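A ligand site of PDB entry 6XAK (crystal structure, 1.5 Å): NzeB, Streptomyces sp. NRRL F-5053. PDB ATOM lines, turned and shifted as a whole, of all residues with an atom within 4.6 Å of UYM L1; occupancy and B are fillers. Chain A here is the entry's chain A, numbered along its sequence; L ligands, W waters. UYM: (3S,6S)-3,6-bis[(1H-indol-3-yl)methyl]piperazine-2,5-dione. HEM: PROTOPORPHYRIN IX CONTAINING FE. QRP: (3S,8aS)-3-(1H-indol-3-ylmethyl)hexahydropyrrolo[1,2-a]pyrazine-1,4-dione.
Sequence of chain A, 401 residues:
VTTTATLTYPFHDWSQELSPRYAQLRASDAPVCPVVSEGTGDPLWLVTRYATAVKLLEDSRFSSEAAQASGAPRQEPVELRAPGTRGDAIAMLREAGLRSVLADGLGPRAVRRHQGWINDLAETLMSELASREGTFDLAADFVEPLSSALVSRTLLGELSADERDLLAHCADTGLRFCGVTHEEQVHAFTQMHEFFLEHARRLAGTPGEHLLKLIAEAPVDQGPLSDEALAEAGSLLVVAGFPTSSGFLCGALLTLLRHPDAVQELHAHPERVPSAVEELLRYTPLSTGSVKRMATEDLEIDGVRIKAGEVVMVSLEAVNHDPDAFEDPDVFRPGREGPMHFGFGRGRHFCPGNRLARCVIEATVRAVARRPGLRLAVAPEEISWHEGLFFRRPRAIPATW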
ATOM      1  N   SER A  64       0.517 -19.676   3.785  1.00  0.00           N
ATOM      2  CA  SER A  64       1.309 -19.831   2.561  1.00  0.00           C
ATOM      3  C   SER A  64       1.847 -18.490   2.086  1.00  0.00           C
ATOM      4  O   SER A  64       3.016 -18.387   1.687  1.00  0.00           O
ATOM      5  CB  SER A  64       0.482 -20.458   1.448  1.00  0.00           C
ATOM      6  OG  SER A  64       1.292 -20.608   0.286  1.00  0.00           O
ATOM      7  N   GLN A  68       5.778 -16.694   1.077  1.00  0.00           N
ATOM      8  CA  GLN A  68       6.138 -16.226  -0.260  1.00  0.00           C
ATOM      9  C   GLN A  68       6.710 -14.811  -0.265  1.00  0.00           C
ATOM     10  O   GLN A  68       7.227 -14.385  -1.304  1.00  0.00           O
ATOM     11  CB  GLN A  68       4.913 -16.255  -1.189  1.00  0.00           C
ATOM     12  CG  GLN A  68       4.255 -17.644  -1.353  1.00  0.00           C
ATOM     13  CD  GLN A  68       2.887 -17.546  -2.021  1.00  0.00           C
ATOM     14  OE1 GLN A  68       2.659 -16.679  -2.872  1.00  0.00           O
ATOM     15  NE2 GLN A  68       1.965 -18.404  -1.614  1.00  0.00           N
ATOM     16  N   LEU A  80      10.947 -15.557  -6.293  1.00  0.00           N
ATOM     17  CA  LEU A  80      10.175 -15.916  -7.483  1.00  0.00           C
ATOM     18  C   LEU A  80       9.301 -14.746  -7.935  1.00  0.00           C
ATOM     19  O   LEU A  80       8.085 -14.812  -7.975  1.00  0.00           O
ATOM     20  CB  LEU A  80       9.345 -17.160  -7.209  1.00  0.00           C
ATOM     21  CG  LEU A  80      10.167 -18.323  -6.662  1.00  0.00           C
ATOM     22  CD1 LEU A  80       9.249 -19.542  -6.457  1.00  0.00           C
ATOM     23  CD2 LEU A  80      11.329 -18.625  -7.583  1.00  0.00           C
ATOM     24  N   ARG A  81       9.973 -13.649  -8.290  1.00  0.00           N
ATOM     25  CA  ARG A  81       9.303 -12.440  -8.729  1.00  0.00           C
ATOM     26  C   ARG A  81      10.344 -11.551  -9.391  1.00  0.00           C
ATOM     27  O   ARG A  81      11.509 -11.523  -8.979  1.00  0.00           O
ATOM     28  CB  ARG A  81       8.687 -11.689  -7.538  1.00  0.00           C
ATOM     29  CG  ARG A  81       9.665 -11.486  -6.370  1.00  0.00           C
ATOM     30  CD  ARG A  81       9.145 -10.520  -5.309  1.00  0.00           C
ATOM     31  NE  ARG A  81       7.931 -10.989  -4.643  1.00  0.00           N
ATOM     32  CZ  ARG A  81       7.885 -11.881  -3.672  1.00  0.00           C
ATOM     33  NH1 ARG A  81       8.996 -12.444  -3.229  1.00  0.00           N
ATOM     34  NH2 ARG A  81       6.721 -12.239  -3.152  1.00  0.00           N
ATOM     35  N   GLY A  87       4.725 -10.047  -6.800  1.00  0.00           N
ATOM     36  CA  GLY A  87       4.698 -11.512  -6.818  1.00  0.00           C
ATOM     37  C   GLY A  87       3.624 -11.987  -5.869  1.00  0.00           C
ATOM     38  O   GLY A  87       3.891 -12.721  -4.916  1.00  0.00           O
ATOM     39  N   ALA A  89       0.030 -12.607  -6.998  1.00  0.00           N
ATOM     40  CA  ALA A  89      -1.004 -12.561  -8.028  1.00  0.00           C
ATOM     41  C   ALA A  89      -2.374 -12.957  -7.501  1.00  0.00           C
ATOM     42  O   ALA A  89      -3.373 -12.296  -7.792  1.00  0.00           O
ATOM     43  CB  ALA A  89      -0.596 -13.432  -9.226  1.00  0.00           C
ATOM     44  N   ILE A  90      -2.458 -14.065  -6.747  1.00  0.00           N
ATOM     45  CA  ILE A  90      -3.748 -14.485  -6.202  1.00  0.00           C
ATOM     46  C   ILE A  90      -4.363 -13.389  -5.350  1.00  0.00           C
ATOM     47  O   ILE A  90      -5.571 -13.118  -5.446  1.00  0.00           O
ATOM     48  CB  ILE A  90      -3.613 -15.819  -5.443  1.00  0.00           C
ATOM     49  CG1 ILE A  90      -3.408 -16.942  -6.456  1.00  0.00           C
ATOM     50  CG2 ILE A  90      -4.856 -16.091  -4.614  1.00  0.00           C
ATOM     51  CD1 ILE A  90      -3.029 -18.257  -5.831  1.00  0.00           C
ATOM     52  N   LEU A 175      12.575 -21.238 -12.332  1.00  0.00           N
ATOM     53  CA  LEU A 175      12.038 -22.244 -11.410  1.00  0.00           C
ATOM     54  C   LEU A 175      13.030 -23.401 -11.272  1.00  0.00           C
ATOM     55  O   LEU A 175      12.792 -24.537 -11.705  1.00  0.00           O
ATOM     56  CB  LEU A 175      10.665 -22.693 -11.895  1.00  0.00           C
ATOM     57  CG  LEU A 175       9.668 -21.548 -12.023  1.00  0.00           C
ATOM     58  CD1 LEU A 175       8.394 -21.996 -12.741  1.00  0.00           C
ATOM     59  CD2 LEU A 175       9.338 -20.946 -10.667  1.00  0.00           C
ATOM     60  N   GLU A 232       1.117  -9.651 -13.513  1.00  0.00           N
ATOM     61  CA  GLU A 232       1.143 -10.604 -12.410  1.00  0.00           C
ATOM     62  C   GLU A 232       0.291 -11.827 -12.713  1.00  0.00           C
ATOM     63  O   GLU A 232       0.689 -12.958 -12.442  1.00  0.00           O
ATOM     64  CB  GLU A 232       0.655  -9.933 -11.122  1.00  0.00           C
ATOM     65  CG  GLU A 232       1.632  -8.906 -10.522  1.00  0.00           C
ATOM     66  CD  GLU A 232       2.449  -9.455  -9.359  1.00  0.00           C
ATOM     67  OE1 GLU A 232       1.884 -10.103  -8.457  1.00  0.00           O
ATOM     68  OE2 GLU A 232       3.683  -9.247  -9.349  1.00  0.00           O
ATOM     69  N   SER A 235       2.075 -13.984 -15.292  1.00  0.00           N
ATOM     70  CA  SER A 235       3.197 -14.666 -14.668  1.00  0.00           C
ATOM     71  C   SER A 235       2.707 -15.864 -13.858  1.00  0.00           C
ATOM     72  O   SER A 235       3.288 -16.954 -13.938  1.00  0.00           O
ATOM     73  CB  SER A 235       3.981 -13.703 -13.776  1.00  0.00           C
ATOM     74  OG  SER A 235       4.726 -12.779 -14.565  1.00  0.00           O
ATOM     75  N   LEU A 236       1.630 -15.673 -13.092  1.00  0.00           N
ATOM     76  CA  LEU A 236       1.058 -16.755 -12.288  1.00  0.00           C
ATOM     77  C   LEU A 236       0.675 -17.950 -13.160  1.00  0.00           C
ATOM     78  O   LEU A 236       1.002 -19.100 -12.833  1.00  0.00           O
ATOM     79  CB  LEU A 236      -0.174 -16.240 -11.549  1.00  0.00           C
ATOM     80  CG  LEU A 236      -1.000 -17.345 -10.884  1.00  0.00           C
ATOM     81  CD1 LEU A 236      -0.166 -18.008  -9.801  1.00  0.00           C
ATOM     82  CD2 LEU A 236      -2.271 -16.766 -10.294  1.00  0.00           C
ATOM     83  N   VAL A 239       3.942 -19.830 -14.316  1.00  0.00           N
ATOM     84  CA  VAL A 239       4.690 -20.581 -13.314  1.00  0.00           C
ATOM     85  C   VAL A 239       3.865 -21.745 -12.764  1.00  0.00           C
ATOM     86  O   VAL A 239       4.410 -22.811 -12.487  1.00  0.00           O
ATOM     87  CB  VAL A 239       5.229 -19.661 -12.196  1.00  0.00           C
ATOM     88  CG1 VAL A 239       6.083 -18.552 -12.759  1.00  0.00           C
ATOM     89  CG2 VAL A 239       4.105 -19.100 -11.352  1.00  0.00           C
ATOM     90  N   ALA A 240       2.551 -21.548 -12.641  1.00  0.00           N
ATOM     91  CA  ALA A 240       1.682 -22.545 -12.018  1.00  0.00           C
ATOM     92  C   ALA A 240       1.166 -23.585 -13.003  1.00  0.00           C
ATOM     93  O   ALA A 240       0.844 -24.709 -12.588  1.00  0.00           O
ATOM     94  CB  ALA A 240       0.517 -21.831 -11.330  1.00  0.00           C
ATOM     95  N   LYS A 292       5.189 -25.093   1.325  1.00  0.00           N
ATOM     96  CA  LYS A 292       5.712 -24.518   2.558  1.00  0.00           C
ATOM     97  C   LYS A 292       4.759 -23.463   3.105  1.00  0.00           C
ATOM     98  O   LYS A 292       4.015 -22.826   2.363  1.00  0.00           O
ATOM     99  CB  LYS A 292       7.140 -23.975   2.356  1.00  0.00           C
ATOM    100  CG  LYS A 292       7.277 -22.589   1.715  1.00  0.00           C
ATOM    101  CD  LYS A 292       6.689 -22.527   0.306  1.00  0.00           C
ATOM    102  CE  LYS A 292       7.147 -21.254  -0.391  1.00  0.00           C
ATOM    103  NZ  LYS A 292       6.424 -21.158  -1.683  1.00  0.00           N
ATOM    104  N   PHE A 391      10.251 -28.576 -10.945  1.00  0.00           N
ATOM    105  CA  PHE A 391       9.265 -29.527 -11.430  1.00  0.00           C
ATOM    106  C   PHE A 391       9.955 -30.455 -12.431  1.00  0.00           C
ATOM    107  O   PHE A 391      10.276 -30.038 -13.555  1.00  0.00           O
ATOM    108  CB  PHE A 391       8.071 -28.797 -12.004  1.00  0.00           C
ATOM    109  CG  PHE A 391       7.445 -27.838 -11.021  1.00  0.00           C
ATOM    110  CD1 PHE A 391       6.776 -28.324  -9.919  1.00  0.00           C
ATOM    111  CD2 PHE A 391       7.576 -26.453 -11.169  1.00  0.00           C
ATOM    112  CE1 PHE A 391       6.201 -27.459  -8.995  1.00  0.00           C
ATOM    113  CE2 PHE A 391       7.000 -25.588 -10.246  1.00  0.00           C
ATOM    114  CZ  PHE A 391       6.319 -26.092  -9.143  1.00  0.00           C
HETATM  115  N   UYM L   1       6.170 -17.009  -8.245  1.00  0.00           N
HETATM  116  C   UYM L   1       1.401 -19.205  -5.821  1.00  0.00           C
HETATM  117  O   UYM L   1       0.394 -18.898  -6.387  1.00  0.00           O
HETATM  118  C1  UYM L   1       2.691 -18.431  -6.143  1.00  0.00           C
HETATM  119  C10 UYM L   1       5.652 -14.846  -9.692  1.00  0.00           C
HETATM  120  C11 UYM L   1       2.529 -20.760  -4.092  1.00  0.00           C
HETATM  121  C12 UYM L   1       2.910 -22.225  -4.451  1.00  0.00           C
HETATM  122  C15 UYM L   1       3.770 -19.899  -4.324  1.00  0.00           C
HETATM  123  C2  UYM L   1       3.068 -18.637  -7.616  1.00  0.00           C
HETATM  124  C3  UYM L   1       4.257 -17.703  -8.059  1.00  0.00           C
HETATM  125  C34 UYM L   1       3.079 -22.524  -5.994  1.00  0.00           C
HETATM  126  C35 UYM L   1       2.053 -22.891  -6.629  1.00  0.00           C
HETATM  127  C37 UYM L   1       3.921 -22.786  -7.950  1.00  0.00           C
HETATM  128  C38 UYM L   1       4.176 -22.441  -6.629  1.00  0.00           C
HETATM  129  C39 UYM L   1       5.491 -22.090  -6.251  1.00  0.00           C
HETATM  130  C4  UYM L   1       5.478 -17.993  -7.709  1.00  0.00           C
HETATM  131  C40 UYM L   1       6.521 -22.070  -7.218  1.00  0.00           C
HETATM  132  C41 UYM L   1       6.248 -22.424  -8.540  1.00  0.00           C
HETATM  133  C42 UYM L   1       4.960 -22.783  -8.915  1.00  0.00           C
HETATM  134  C5  UYM L   1       5.437 -16.025  -8.973  1.00  0.00           C
HETATM  135  C6  UYM L   1       4.106 -16.557  -8.804  1.00  0.00           C
HETATM  136  C7  UYM L   1       3.048 -15.848  -9.385  1.00  0.00           C
HETATM  137  C8  UYM L   1       3.258 -14.660 -10.106  1.00  0.00           C
HETATM  138  C9  UYM L   1       4.566 -14.150 -10.264  1.00  0.00           C
HETATM  139  N1  UYM L   1       3.790 -18.826  -5.291  1.00  0.00           N
HETATM  140  N2  UYM L   1       1.394 -20.281  -4.842  1.00  0.00           N
HETATM  141  N36 UYM L   1       2.456 -23.091  -7.970  1.00  0.00           N
HETATM  142  O1  UYM L   1       4.738 -20.115  -3.678  1.00  0.00           O
HETATM  143  CHA HEM L   2      -1.309 -24.955  -6.540  1.00  0.00           C
HETATM  144  CHB HEM L   2      -0.168 -29.365  -8.229  1.00  0.00           C
HETATM  145  CHC HEM L   2      -1.493 -28.011 -12.705  1.00  0.00           C
HETATM  146  CHD HEM L   2      -2.746 -23.629 -10.952  1.00  0.00           C
HETATM  147  C1A HEM L   2      -0.912 -26.275  -6.607  1.00  0.00           C
HETATM  148  C2A HEM L   2      -0.450 -27.070  -5.493  1.00  0.00           C
HETATM  149  C3A HEM L   2      -0.133 -28.274  -5.957  1.00  0.00           C
HETATM  150  C4A HEM L   2      -0.372 -28.296  -7.393  1.00  0.00           C
HETATM  151  CMA HEM L   2       0.404 -29.434  -5.100  1.00  0.00           C
HETATM  152  CAA HEM L   2      -0.375 -26.673  -3.999  1.00  0.00           C
HETATM  153  CBA HEM L   2       0.792 -25.756  -3.637  1.00  0.00           C
HETATM  154  CGA HEM L   2       0.785 -25.415  -2.165  1.00  0.00           C
HETATM  155  O1A HEM L   2       0.061 -26.055  -1.357  1.00  0.00           O
HETATM  156  O2A HEM L   2       1.518 -24.469  -1.769  1.00  0.00           O
HETATM  157  C1B HEM L   2      -0.426 -29.376  -9.587  1.00  0.00           C
HETATM  158  C2B HEM L   2      -0.222 -30.528 -10.456  1.00  0.00           C
HETATM  159  C3B HEM L   2      -0.572 -30.134 -11.712  1.00  0.00           C
HETATM  160  C4B HEM L   2      -1.033 -28.755 -11.635  1.00  0.00           C
HETATM  161  CMB HEM L   2       0.345 -31.872  -9.945  1.00  0.00           C
HETATM  162  CAB HEM L   2      -0.569 -30.955 -13.026  1.00  0.00           C
HETATM  163  CBB HEM L   2      -0.504 -32.292 -13.037  1.00  0.00           C
HETATM  164  C1C HEM L   2      -1.954 -26.699 -12.612  1.00  0.00           C
HETATM  165  C2C HEM L   2      -2.466 -25.917 -13.709  1.00  0.00           C
HETATM  166  C3C HEM L   2      -2.784 -24.713 -13.245  1.00  0.00           C
HETATM  167  C4C HEM L   2      -2.517 -24.678 -11.818  1.00  0.00           C
HETATM  168  CMC HEM L   2      -2.575 -26.427 -15.157  1.00  0.00           C
HETATM  169  CAC HEM L   2      -3.373 -23.582 -14.124  1.00  0.00           C
HETATM  170  CBC HEM L   2      -3.040 -22.304 -13.956  1.00  0.00           C
HETATM  171  C1D HEM L   2      -2.378 -23.565  -9.630  1.00  0.00           C
HETATM  172  C2D HEM L   2      -2.333 -22.369  -8.805  1.00  0.00           C
HETATM  173  C3D HEM L   2      -1.909 -22.729  -7.576  1.00  0.00           C
HETATM  174  C4D HEM L   2      -1.703 -24.164  -7.599  1.00  0.00           C
HETATM  175  CMD HEM L   2      -2.667 -20.934  -9.275  1.00  0.00           C
HETATM  176  CAD HEM L   2      -1.658 -21.829  -6.329  1.00  0.00           C
HETATM  177  CBD HEM L   2      -2.826 -21.821  -5.375  1.00  0.00           C
HETATM  178  CGD HEM L   2      -2.460 -21.213  -4.036  1.00  0.00           C
HETATM  179  O1D HEM L   2      -1.267 -20.947  -3.741  1.00  0.00           O
HETATM  180  O2D HEM L   2      -3.405 -20.972  -3.243  1.00  0.00           O
HETATM  181  NA  HEM L   2      -0.851 -27.046  -7.750  1.00  0.00           N
HETATM  182  NB  HEM L   2      -0.913 -28.301 -10.333  1.00  0.00           N
HETATM  183  NC  HEM L   2      -2.021 -25.918 -11.461  1.00  0.00           N
HETATM  184  ND  HEM L   2      -1.993 -24.643  -8.852  1.00  0.00           N
HETATM  185 FE   HEM L   2      -1.689 -26.584  -9.552  1.00  0.00          FE
HETATM  186  C   QRP L   3       6.860 -24.275  -4.011  1.00  0.00           C
HETATM  187  N   QRP L   3       7.280 -26.356  -5.254  1.00  0.00           N
HETATM  188  O   QRP L   3       6.197 -23.713  -3.161  1.00  0.00           O
HETATM  189  CA  QRP L   3       6.273 -25.408  -4.804  1.00  0.00           C
HETATM  190  CB  QRP L   3       5.184 -26.148  -4.016  1.00  0.00           C
HETATM  191  CG  QRP L   3       4.800 -27.390  -4.804  1.00  0.00           C
HETATM  192  OAA QRP L   3       9.371 -26.807  -6.041  1.00  0.00           O
HETATM  193  CAH QRP L   3      10.253 -22.930  -4.283  1.00  0.00           C
HETATM  194  CAI QRP L   3      10.330 -24.363  -4.778  1.00  0.00           C
HETATM  195  CAJ QRP L   3       8.853 -22.799  -3.668  1.00  0.00           C
HETATM  196  CAN QRP L   3       8.550 -26.022  -5.573  1.00  0.00           C
HETATM  197  CAT QRP L   3       8.917 -24.578  -5.305  1.00  0.00           C
HETATM  198  NAU QRP L   3       8.105 -23.894  -4.305  1.00  0.00           N
HETATM  199  CD1 QRP L   3       5.131 -28.681  -4.436  1.00  0.00           C
HETATM  200  CD2 QRP L   3       4.096 -27.489  -6.009  1.00  0.00           C
HETATM  201  NE1 QRP L   3       4.629 -29.558  -5.353  1.00  0.00           N
HETATM  202  CE2 QRP L   3       4.018 -28.855  -6.311  1.00  0.00           C
HETATM  203  CE3 QRP L   3       3.529 -26.534  -6.842  1.00  0.00           C
HETATM  204  CH2 QRP L   3       2.803 -28.326  -8.299  1.00  0.00           C
HETATM  205  CZ2 QRP L   3       3.370 -29.281  -7.465  1.00  0.00           C
HETATM  206  CZ3 QRP L   3       2.867 -26.955  -7.988  1.00  0.00           C
HETATM  207  O   HOH W   1      -0.147 -16.155  -6.564  1.00  0.00           O
HETATM  208  O   HOH W   2       3.769 -21.134  -0.716  1.00  0.00           O
HETATM  209  O   HOH W   3       2.112 -14.722  -6.981  1.00  0.00           O
HETATM  210  O   HOH W   4       6.513 -14.903  -5.716  1.00  0.00           O
HETATM  211  O   HOH W   5       0.865 -24.798  -9.803  1.00  0.00           O
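An oxygen (O1) of UYM L1 is in hydrogen-bond range of the side-chain amino group (NZ) of Lys 292, 2.8 Å away. A nitrogen (N) of UYM L1 sits at hydrogen-bond distance from the backbone carbonyl oxygen (O) of Leu 80. N1 of UYM L1 is in hydrogen-bond range of OE1 of Gln 68. An oxygen (O) of QRP L3 sits at hydrogen-bond distance from the side-chain amino group of Lys 292, at 3.0 Å.
N2 of UYM L1 is in hydrogen-bond range of O1D of HEM L2 (3.0 Å).
The backbone carbonyl oxygen (O) of Gln 68 lies within hydrogen-bond range of the guanidinium group (NH2) of Arg 81 (2.9 Å). The side-chain amide nitrogen (NE2) of Gln 68 lies within hydrogen-bond range of the side-chain hydroxyl (OG) of Ser 64 (3.0 Å). N of Ala 89 lies within hydrogen-bond range of OE1 of Glu 232 (3.4 Å). OE2 of Glu 232 sits at hydrogen-bond distance from N of Gly 87 (2.9 Å).
CD1 of Ile 90 touches O of UYM L1 (3.5 Å). Glu 232 touches UYM L1. Ser 235 touches UYM L1. N of Leu 236 touches C8 of UYM L1, 3.5 Å away. CG2 of Val 239 touches C3 of UYM L1, 3.6 Å away. CZ of Phe 391 touches C42 of UYM L1, at 3.6 Å. Within 4 Å of UYM L1: Gln 68, Leu 80, Ile 90, Glu 232, Ser 235, Leu 236, Val 239, Lys 292 and Phe 391. The nearest printed residue that does not touch UYM L1 is Leu 175 (4.03 Å).
Water W1 lies within hydrogen-bond range of O of UYM L1 (2.8 Å) and N of Ile 90 (3.1 Å). Water W5 lies within hydrogen-bond range of the backbone carbonyl oxygen (O) of Ala 240 (2.8 Å) and a nitrogen (N36) of UYM L1 (3.0 Å). Water W2 lies within hydrogen-bond range of OG of Ser 64 (2.7 Å), NZ of Lys 292 (2.8 Å), O1 of UYM L1 (3.3 Å) and NE2 of Gln 68 (3.4 Å). Water W4 lies within hydrogen-bond range of O of Leu 80 (2.8 Å) and N of UYM L1 (3.3 Å).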
